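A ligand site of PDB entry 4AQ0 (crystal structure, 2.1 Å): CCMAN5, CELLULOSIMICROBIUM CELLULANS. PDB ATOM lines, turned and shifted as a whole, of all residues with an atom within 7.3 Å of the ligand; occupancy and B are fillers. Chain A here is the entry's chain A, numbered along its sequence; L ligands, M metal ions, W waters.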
ATOM      1  N   ASN A  65       6.045 -25.102  -9.536  1.00  0.00           N
ATOM      2  CA  ASN A  65       6.547 -25.116 -10.919  1.00  0.00           C
ATOM      3  C   ASN A  65       8.053 -25.398 -11.046  1.00  0.00           C
ATOM      4  O   ASN A  65       8.499 -25.925 -12.057  1.00  0.00           O
ATOM      5  CB  ASN A  65       6.177 -23.802 -11.644  1.00  0.00           C
ATOM      6  CG  ASN A  65       4.658 -23.553 -11.711  1.00  0.00           C
ATOM      7  OD1 ASN A  65       3.870 -24.587 -11.476  1.00  0.00           O
ATOM      8  ND2 ASN A  65       4.220 -22.438 -12.005  1.00  0.00           N
ATOM      9  N   LEU A  83      13.796 -22.393 -14.138  1.00  0.00           N
ATOM     10  CA  LEU A  83      13.383 -20.991 -14.313  1.00  0.00           C
ATOM     11  C   LEU A  83      12.712 -20.514 -13.039  1.00  0.00           C
ATOM     12  O   LEU A  83      11.866 -21.223 -12.494  1.00  0.00           O
ATOM     13  CB  LEU A  83      12.381 -20.879 -15.469  1.00  0.00           C
ATOM     14  CG  LEU A  83      12.903 -21.234 -16.865  1.00  0.00           C
ATOM     15  CD1 LEU A  83      11.782 -21.096 -17.896  1.00  0.00           C
ATOM     16  CD2 LEU A  83      14.077 -20.375 -17.228  1.00  0.00           C
ATOM     17  N   ASP A  84      13.076 -19.321 -12.566  1.00  0.00           N
ATOM     18  CA  ASP A  84      12.532 -18.773 -11.318  1.00  0.00           C
ATOM     19  C   ASP A  84      11.178 -18.106 -11.489  1.00  0.00           C
ATOM     20  O   ASP A  84      11.017 -17.212 -12.316  1.00  0.00           O
ATOM     21  CB  ASP A  84      13.507 -17.766 -10.688  1.00  0.00           C
ATOM     22  CG  ASP A  84      14.892 -18.336 -10.484  1.00  0.00           C
ATOM     23  OD1 ASP A  84      15.631 -18.447 -11.476  1.00  0.00           O
ATOM     24  OD2 ASP A  84      15.246 -18.672  -9.324  1.00  0.00           O
ATOM     25  N   GLY A  85      10.190 -18.544 -10.696  1.00  0.00           N
ATOM     26  CA  GLY A  85       8.911 -17.846 -10.574  1.00  0.00           C
ATOM     27  C   GLY A  85       8.017 -17.831 -11.793  1.00  0.00           C
ATOM     28  O   GLY A  85       7.114 -16.989 -11.895  1.00  0.00           O
ATOM     29  N   VAL A  86       8.229 -18.756 -12.720  1.00  0.00           N
ATOM     30  CA  VAL A  86       7.430 -18.765 -13.951  1.00  0.00           C
ATOM     31  C   VAL A  86       6.127 -19.560 -13.792  1.00  0.00           C
ATOM     32  O   VAL A  86       5.946 -20.284 -12.793  1.00  0.00           O
ATOM     33  CB  VAL A  86       8.239 -19.231 -15.186  1.00  0.00           C
ATOM     34  CG1 VAL A  86       9.393 -18.277 -15.440  1.00  0.00           C
ATOM     35  CG2 VAL A  86       8.733 -20.649 -15.018  1.00  0.00           C
ATOM     36  N   GLY A  87       5.247 -19.426 -14.790  1.00  0.00           N
ATOM     37  CA  GLY A  87       3.920 -20.063 -14.752  1.00  0.00           C
ATOM     38  C   GLY A  87       3.885 -21.407 -15.458  1.00  0.00           C
ATOM     39  O   GLY A  87       4.908 -22.107 -15.519  1.00  0.00           O
ATOM     40  N   GLY A  88       2.722 -21.770 -15.993  1.00  0.00           N
ATOM     41  CA  GLY A  88       2.528 -23.098 -16.585  1.00  0.00           C
ATOM     42  C   GLY A  88       2.838 -24.167 -15.552  1.00  0.00           C
ATOM     43  O   GLY A  88       2.359 -24.116 -14.413  1.00  0.00           O
ATOM     44  N   SER A  89       3.646 -25.154 -15.933  1.00  0.00           N
ATOM     45  CA  SER A  89       4.093 -26.172 -14.991  1.00  0.00           C
ATOM     46  C   SER A  89       5.597 -26.031 -14.763  1.00  0.00           C
ATOM     47  O   SER A  89       6.256 -26.948 -14.230  1.00  0.00           O
ATOM     48  CB  SER A  89       3.691 -27.579 -15.465  1.00  0.00           C
ATOM     49  OG  SER A  89       4.395 -27.947 -16.645  1.00  0.00           O
ATOM     50  N   GLY A  90       6.125 -24.876 -15.144  1.00  0.00           N
ATOM     51  CA  GLY A  90       7.540 -24.555 -14.930  1.00  0.00           C
ATOM     52  C   GLY A  90       8.453 -24.978 -16.081  1.00  0.00           C
ATOM     53  O   GLY A  90       8.105 -25.839 -16.876  1.00  0.00           O
ATOM     54  N   PHE A 211       9.728 -24.948 -23.054  1.00  0.00           N
ATOM     55  CA  PHE A 211       8.857 -24.178 -22.186  1.00  0.00           C
ATOM     56  C   PHE A 211       8.229 -22.997 -22.919  1.00  0.00           C
ATOM     57  O   PHE A 211       8.937 -22.176 -23.516  1.00  0.00           O
ATOM     58  CB  PHE A 211       9.583 -23.682 -20.919  1.00  0.00           C
ATOM     59  CG  PHE A 211       8.684 -22.904 -19.973  1.00  0.00           C
ATOM     60  CD1 PHE A 211       7.679 -23.556 -19.248  1.00  0.00           C
ATOM     61  CD2 PHE A 211       8.814 -21.523 -19.826  1.00  0.00           C
ATOM     62  CE1 PHE A 211       6.843 -22.854 -18.385  1.00  0.00           C
ATOM     63  CE2 PHE A 211       7.976 -20.801 -18.960  1.00  0.00           C
ATOM     64  CZ  PHE A 211       6.999 -21.461 -18.246  1.00  0.00           C
ATOM     65  N   TYR A 212       6.909 -22.929 -22.858  1.00  0.00           N
ATOM     66  CA  TYR A 212       6.097 -21.810 -23.366  1.00  0.00           C
ATOM     67  C   TYR A 212       6.191 -21.582 -24.883  1.00  0.00           C
ATOM     68  O   TYR A 212       5.367 -22.119 -25.627  1.00  0.00           O
ATOM     69  CB  TYR A 212       6.303 -20.513 -22.558  1.00  0.00           C
ATOM     70  CG  TYR A 212       5.224 -19.486 -22.810  1.00  0.00           C
ATOM     71  CD1 TYR A 212       3.888 -19.736 -22.449  1.00  0.00           C
ATOM     72  CD2 TYR A 212       5.521 -18.285 -23.440  1.00  0.00           C
ATOM     73  CE1 TYR A 212       2.885 -18.797 -22.700  1.00  0.00           C
ATOM     74  CE2 TYR A 212       4.535 -17.333 -23.703  1.00  0.00           C
ATOM     75  CZ  TYR A 212       3.217 -17.604 -23.335  1.00  0.00           C
ATOM     76  OH  TYR A 212       2.241 -16.662 -23.595  1.00  0.00           O
ATOM     77  N   ALA A 368      11.755 -13.252 -20.035  1.00  0.00           N
ATOM     78  CA  ALA A 368      10.309 -13.304 -19.821  1.00  0.00           C
ATOM     79  C   ALA A 368       9.811 -11.860 -19.827  1.00  0.00           C
ATOM     80  O   ALA A 368       9.155 -11.403 -18.890  1.00  0.00           O
ATOM     81  CB  ALA A 368      10.001 -13.992 -18.482  1.00  0.00           C
ATOM     82  N   THR A 369      10.124 -11.168 -20.911  1.00  0.00           N
ATOM     83  CA  THR A 369      10.145  -9.711 -20.899  1.00  0.00           C
ATOM     84  C   THR A 369       8.753  -9.069 -20.844  1.00  0.00           C
ATOM     85  O   THR A 369       8.605  -7.956 -20.341  1.00  0.00           O
ATOM     86  CB  THR A 369      11.066  -9.184 -22.041  1.00  0.00           C
ATOM     87  OG1 THR A 369      12.325  -9.885 -21.947  1.00  0.00           O
ATOM     88  CG2 THR A 369      11.344  -7.705 -21.892  1.00  0.00           C
ATOM     89  N   TRP A 370       7.745  -9.786 -21.327  1.00  0.00           N
ATOM     90  CA  TRP A 370       6.336  -9.376 -21.207  1.00  0.00           C
ATOM     91  C   TRP A 370       5.931  -9.158 -19.739  1.00  0.00           C
ATOM     92  O   TRP A 370       5.180  -8.218 -19.428  1.00  0.00           O
ATOM     93  CB  TRP A 370       5.441 -10.440 -21.840  1.00  0.00           C
ATOM     94  CG  TRP A 370       4.005 -10.031 -22.064  1.00  0.00           C
ATOM     95  CD1 TRP A 370       3.498  -9.416 -23.174  1.00  0.00           C
ATOM     96  CD2 TRP A 370       2.898 -10.246 -21.180  1.00  0.00           C
ATOM     97  NE1 TRP A 370       2.148  -9.221 -23.027  1.00  0.00           N
ATOM     98  CE2 TRP A 370       1.753  -9.723 -21.815  1.00  0.00           C
ATOM     99  CE3 TRP A 370       2.765 -10.825 -19.915  1.00  0.00           C
ATOM    100  CZ2 TRP A 370       0.480  -9.759 -21.236  1.00  0.00           C
ATOM    101  CZ3 TRP A 370       1.497 -10.863 -19.322  1.00  0.00           C
ATOM    102  CH2 TRP A 370       0.379 -10.333 -19.988  1.00  0.00           C
ATOM    103  N   ASP A 371       6.434 -10.013 -18.855  1.00  0.00           N
ATOM    104  CA  ASP A 371       6.204  -9.904 -17.407  1.00  0.00           C
ATOM    105  C   ASP A 371       7.200  -8.999 -16.693  1.00  0.00           C
ATOM    106  O   ASP A 371       6.828  -8.287 -15.749  1.00  0.00           O
ATOM    107  CB  ASP A 371       6.288 -11.294 -16.740  1.00  0.00           C
ATOM    108  CG  ASP A 371       5.359 -12.319 -17.372  1.00  0.00           C
ATOM    109  OD1 ASP A 371       4.118 -12.109 -17.348  1.00  0.00           O
ATOM    110  OD2 ASP A 371       5.870 -13.332 -17.876  1.00  0.00           O
ATOM    111  N   VAL A 420      11.506 -17.904 -21.991  1.00  0.00           N
ATOM    112  CA  VAL A 420      10.056 -17.727 -21.956  1.00  0.00           C
ATOM    113  C   VAL A 420       9.504 -16.903 -23.121  1.00  0.00           C
ATOM    114  O   VAL A 420       8.902 -17.465 -24.040  1.00  0.00           O
ATOM    115  CB  VAL A 420       9.550 -17.152 -20.603  1.00  0.00           C
ATOM    116  CG1 VAL A 420       8.022 -17.249 -20.518  1.00  0.00           C
ATOM    117  CG2 VAL A 420      10.183 -17.880 -19.437  1.00  0.00           C
ATOM    118  N   ARG A 421       9.697 -15.595 -23.080  1.00  0.00           N
ATOM    119  CA  ARG A 421       9.095 -14.697 -24.076  1.00  0.00           C
ATOM    120  C   ARG A 421       9.829 -13.345 -24.147  1.00  0.00           C
ATOM    121  O   ARG A 421      10.589 -12.997 -23.241  1.00  0.00           O
ATOM    122  CB  ARG A 421       7.592 -14.521 -23.783  1.00  0.00           C
ATOM    123  CG  ARG A 421       7.285 -13.787 -22.483  1.00  0.00           C
ATOM    124  CD  ARG A 421       5.834 -13.980 -22.068  1.00  0.00           C
ATOM    125  NE  ARG A 421       4.874 -13.484 -23.067  1.00  0.00           N
ATOM    126  CZ  ARG A 421       3.565 -13.405 -22.874  1.00  0.00           C
ATOM    127  NH1 ARG A 421       3.039 -13.765 -21.705  1.00  0.00           N
ATOM    128  NH2 ARG A 421       2.777 -12.946 -23.837  1.00  0.00           N
ATOM    129  N   GLU A 423       8.424 -10.075 -25.647  1.00  0.00           N
ATOM    130  CA  GLU A 423       7.703  -8.803 -25.798  1.00  0.00           C
ATOM    131  C   GLU A 423       8.259  -7.755 -24.830  1.00  0.00           C
ATOM    132  O   GLU A 423       8.691  -8.098 -23.734  1.00  0.00           O
ATOM    133  CB  GLU A 423       6.195  -8.973 -25.556  1.00  0.00           C
ATOM    134  CG  GLU A 423       5.512 -10.008 -26.450  1.00  0.00           C
ATOM    135  CD  GLU A 423       5.362 -11.378 -25.786  1.00  0.00           C
ATOM    136  OE1 GLU A 423       6.126 -11.701 -24.857  1.00  0.00           O
ATOM    137  OE2 GLU A 423       4.462 -12.131 -26.197  1.00  0.00           O
ATOM    138  N   TYR A 551      -5.456  -9.642 -21.390  1.00  0.00           N
ATOM    139  CA  TYR A 551      -4.749 -10.753 -20.763  1.00  0.00           C
ATOM    140  C   TYR A 551      -4.345 -10.417 -19.337  1.00  0.00           C
ATOM    141  O   TYR A 551      -3.609  -9.465 -19.101  1.00  0.00           O
ATOM    142  CB  TYR A 551      -3.520 -11.144 -21.610  1.00  0.00           C
ATOM    143  CG  TYR A 551      -3.861 -12.029 -22.792  1.00  0.00           C
ATOM    144  CD1 TYR A 551      -4.274 -11.482 -24.024  1.00  0.00           C
ATOM    145  CD2 TYR A 551      -3.779 -13.425 -22.695  1.00  0.00           C
ATOM    146  CE1 TYR A 551      -4.588 -12.306 -25.125  1.00  0.00           C
ATOM    147  CE2 TYR A 551      -4.093 -14.263 -23.775  1.00  0.00           C
ATOM    148  CZ  TYR A 551      -4.498 -13.700 -24.978  1.00  0.00           C
ATOM    149  OH  TYR A 551      -4.802 -14.551 -26.033  1.00  0.00           O
ATOM    150  N   GLN A 552      -4.862 -11.201 -18.385  1.00  0.00           N
ATOM    151  CA  GLN A 552      -4.467 -11.137 -16.976  1.00  0.00           C
ATOM    152  C   GLN A 552      -4.679  -9.767 -16.313  1.00  0.00           C
ATOM    153  O   GLN A 552      -3.872  -9.346 -15.473  1.00  0.00           O
ATOM    154  CB  GLN A 552      -3.003 -11.562 -16.831  1.00  0.00           C
ATOM    155  CG  GLN A 552      -2.765 -13.049 -16.625  1.00  0.00           C
ATOM    156  CD  GLN A 552      -1.306 -13.327 -16.309  1.00  0.00           C
ATOM    157  OE1 GLN A 552      -0.436 -13.121 -17.146  1.00  0.00           O
ATOM    158  NE2 GLN A 552      -1.024 -13.759 -15.078  1.00  0.00           N
ATOM    159  N   THR A 642      -4.976 -14.821 -12.072  1.00  0.00           N
ATOM    160  CA  THR A 642      -5.586 -15.764 -13.016  1.00  0.00           C
ATOM    161  C   THR A 642      -7.069 -15.951 -12.650  1.00  0.00           C
ATOM    162  O   THR A 642      -7.513 -15.457 -11.621  1.00  0.00           O
ATOM    163  CB  THR A 642      -4.788 -17.117 -13.044  1.00  0.00           C
ATOM    164  OG1 THR A 642      -5.149 -17.875 -14.203  1.00  0.00           O
ATOM    165  CG2 THR A 642      -5.016 -17.943 -11.780  1.00  0.00           C
ATOM    166  N   ASP A 676       2.932 -15.161  -9.145  1.00  0.00           N
ATOM    167  CA  ASP A 676       4.233 -15.673  -9.566  1.00  0.00           C
ATOM    168  C   ASP A 676       5.258 -14.551  -9.493  1.00  0.00           C
ATOM    169  O   ASP A 676       4.935 -13.402  -9.768  1.00  0.00           O
ATOM    170  CB  ASP A 676       4.151 -16.204 -10.997  1.00  0.00           C
ATOM    171  CG  ASP A 676       3.293 -17.443 -11.117  1.00  0.00           C
ATOM    172  OD1 ASP A 676       3.204 -18.211 -10.124  1.00  0.00           O
ATOM    173  OD2 ASP A 676       2.718 -17.665 -12.203  1.00  0.00           O
ATOM    174  N   ASP A 678       7.888 -14.332 -11.402  1.00  0.00           N
ATOM    175  CA  ASP A 678       8.175 -14.059 -12.811  1.00  0.00           C
ATOM    176  C   ASP A 678       9.611 -13.593 -13.027  1.00  0.00           C
ATOM    177  O   ASP A 678       9.862 -12.396 -13.237  1.00  0.00           O
ATOM    178  CB  ASP A 678       7.178 -13.056 -13.424  1.00  0.00           C
ATOM    179  CG  ASP A 678       5.770 -13.632 -13.554  1.00  0.00           C
ATOM    180  OD1 ASP A 678       5.585 -14.677 -14.216  1.00  0.00           O
ATOM    181  OD2 ASP A 678       4.834 -13.023 -12.985  1.00  0.00           O
ATOM    182  N   ALA A 679      10.551 -14.536 -12.980  1.00  0.00           N
ATOM    183  CA  ALA A 679      11.959 -14.230 -13.216  1.00  0.00           C
ATOM    184  C   ALA A 679      12.486 -13.132 -12.255  1.00  0.00           C
ATOM    185  O   ALA A 679      13.312 -12.305 -12.643  1.00  0.00           O
ATOM    186  CB  ALA A 679      12.178 -13.830 -14.684  1.00  0.00           C
HETATM  187  C1  LIG L   1       0.541 -16.605 -19.134  1.00  0.00           C
HETATM  188  C2  LIG L   1      -0.454 -17.611 -19.502  1.00  0.00           C
HETATM  189  C3  LIG L   1       1.898 -16.954 -19.612  1.00  0.00           C
HETATM  190  N1  LIG L   1       2.692 -16.813 -18.451  1.00  0.00           N
HETATM  191  C4  LIG L   1       4.050 -17.132 -18.445  1.00  0.00           C
HETATM  192  C5  LIG L   1       4.566 -16.882 -17.022  1.00  0.00           C
HETATM  193  C6  LIG L   1       4.159 -18.596 -18.847  1.00  0.00           C
HETATM  194  C7  LIG L   1       4.737 -16.156 -19.413  1.00  0.00           C
HETATM  195  O1  LIG L   1       5.783 -17.497 -16.843  1.00  0.00           O
HETATM  196  O2  LIG L   1       3.514 -19.404 -17.908  1.00  0.00           O
HETATM  197  O3  LIG L   1       4.205 -14.877 -19.272  1.00  0.00           O
HETATM  198 CA    CA M   1       2.453 -12.491 -13.265  1.00  0.00          CA
HETATM  199  O   HOH W   1       0.556 -19.937 -16.165  1.00  0.00           O
HETATM  200  O   HOH W   2       3.166 -16.077 -14.234  1.00  0.00           O
HETATM  201  O   HOH W   3       1.265 -17.461 -15.907  1.00  0.00           O
HETATM  202  O   HOH W   4       2.132 -14.316 -17.113  1.00  0.00           O
HETATM  203  O   HOH W   5       7.206 -15.073 -16.204  1.00  0.00           O
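NE of Arg 421 is in salt-bridge range of OE1 of Glu 423 (2.8 Å).
The side-chain amide oxygen of Asn 65 lies close to the backbone carbonyl oxygen of Gly 88.
O of Arg 421 is in hydrogen-bond range of N of Thr 369, at 3.0 Å.
N of Asp 678 is in hydrogen-bond range of O of Gly 85 (2.8 Å).
The backbone carbonyl oxygen (O) of Val 86 is in hydrogen-bond range of the side-chain amide nitrogen (ND2) of Asn 65.
The backbone carbonyl oxygen (O) of Arg 421 lies within hydrogen-bond range of the backbone NH (N) of Ala 368, at 3.4 Å.
Merely in contact with the ligand: Val 86 (3.4 Å), Val 420 (3.6 Å), Asp 678 (3.7 Å) and Tyr 212 (3.7 Å).
Hydrophobic or aromatic side chains that line the ligand: Val 86, Tyr 212 and Val 420.
Of the 24 residues printed, 8 come within 4 Å of the ligand.
Along chain A the residues within 4 Å of the ligand span positions 86 to 678.
The nearest printed residue that does not touch the ligand is Phe 211 (4.1 Å).
Water W5 lies within hydrogen-bond range of OD1 of Asp 678 (2.6 Å), OD2 of Asp 371 (2.8 Å) and O1 of the ligand (2.9 Å).
Water W4 lies within hydrogen-bond range of the side-chain amide oxygen of Gln 552, a nitrogen (N1) of the ligand and the side-chain carboxylate of Asp 371.
Water W2 lies within hydrogen-bond range of the side-chain carboxylate (OD2) of Asp 676 (2.6 Å) and the side-chain carboxylate (OD1) of Asp 678 (2.8 Å).
Water W1 lies within hydrogen-bond range of N of Gly 88 and O2 of the ligand.
The guanidinium group (NH1) of Arg 421 lies within hydrogen-bond range of an oxygen (O3) of the ligand, at 2.9 Å.
N of Gly 88 sits at hydrogen-bond distance from O2 of the ligand (3.1 Å).
OD2 of Asp 371 lies within hydrogen-bond range of O3 of the ligand, at 2.7 Å.
N of Gly 87 sits at hydrogen-bond distance from O1 of the ligand.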
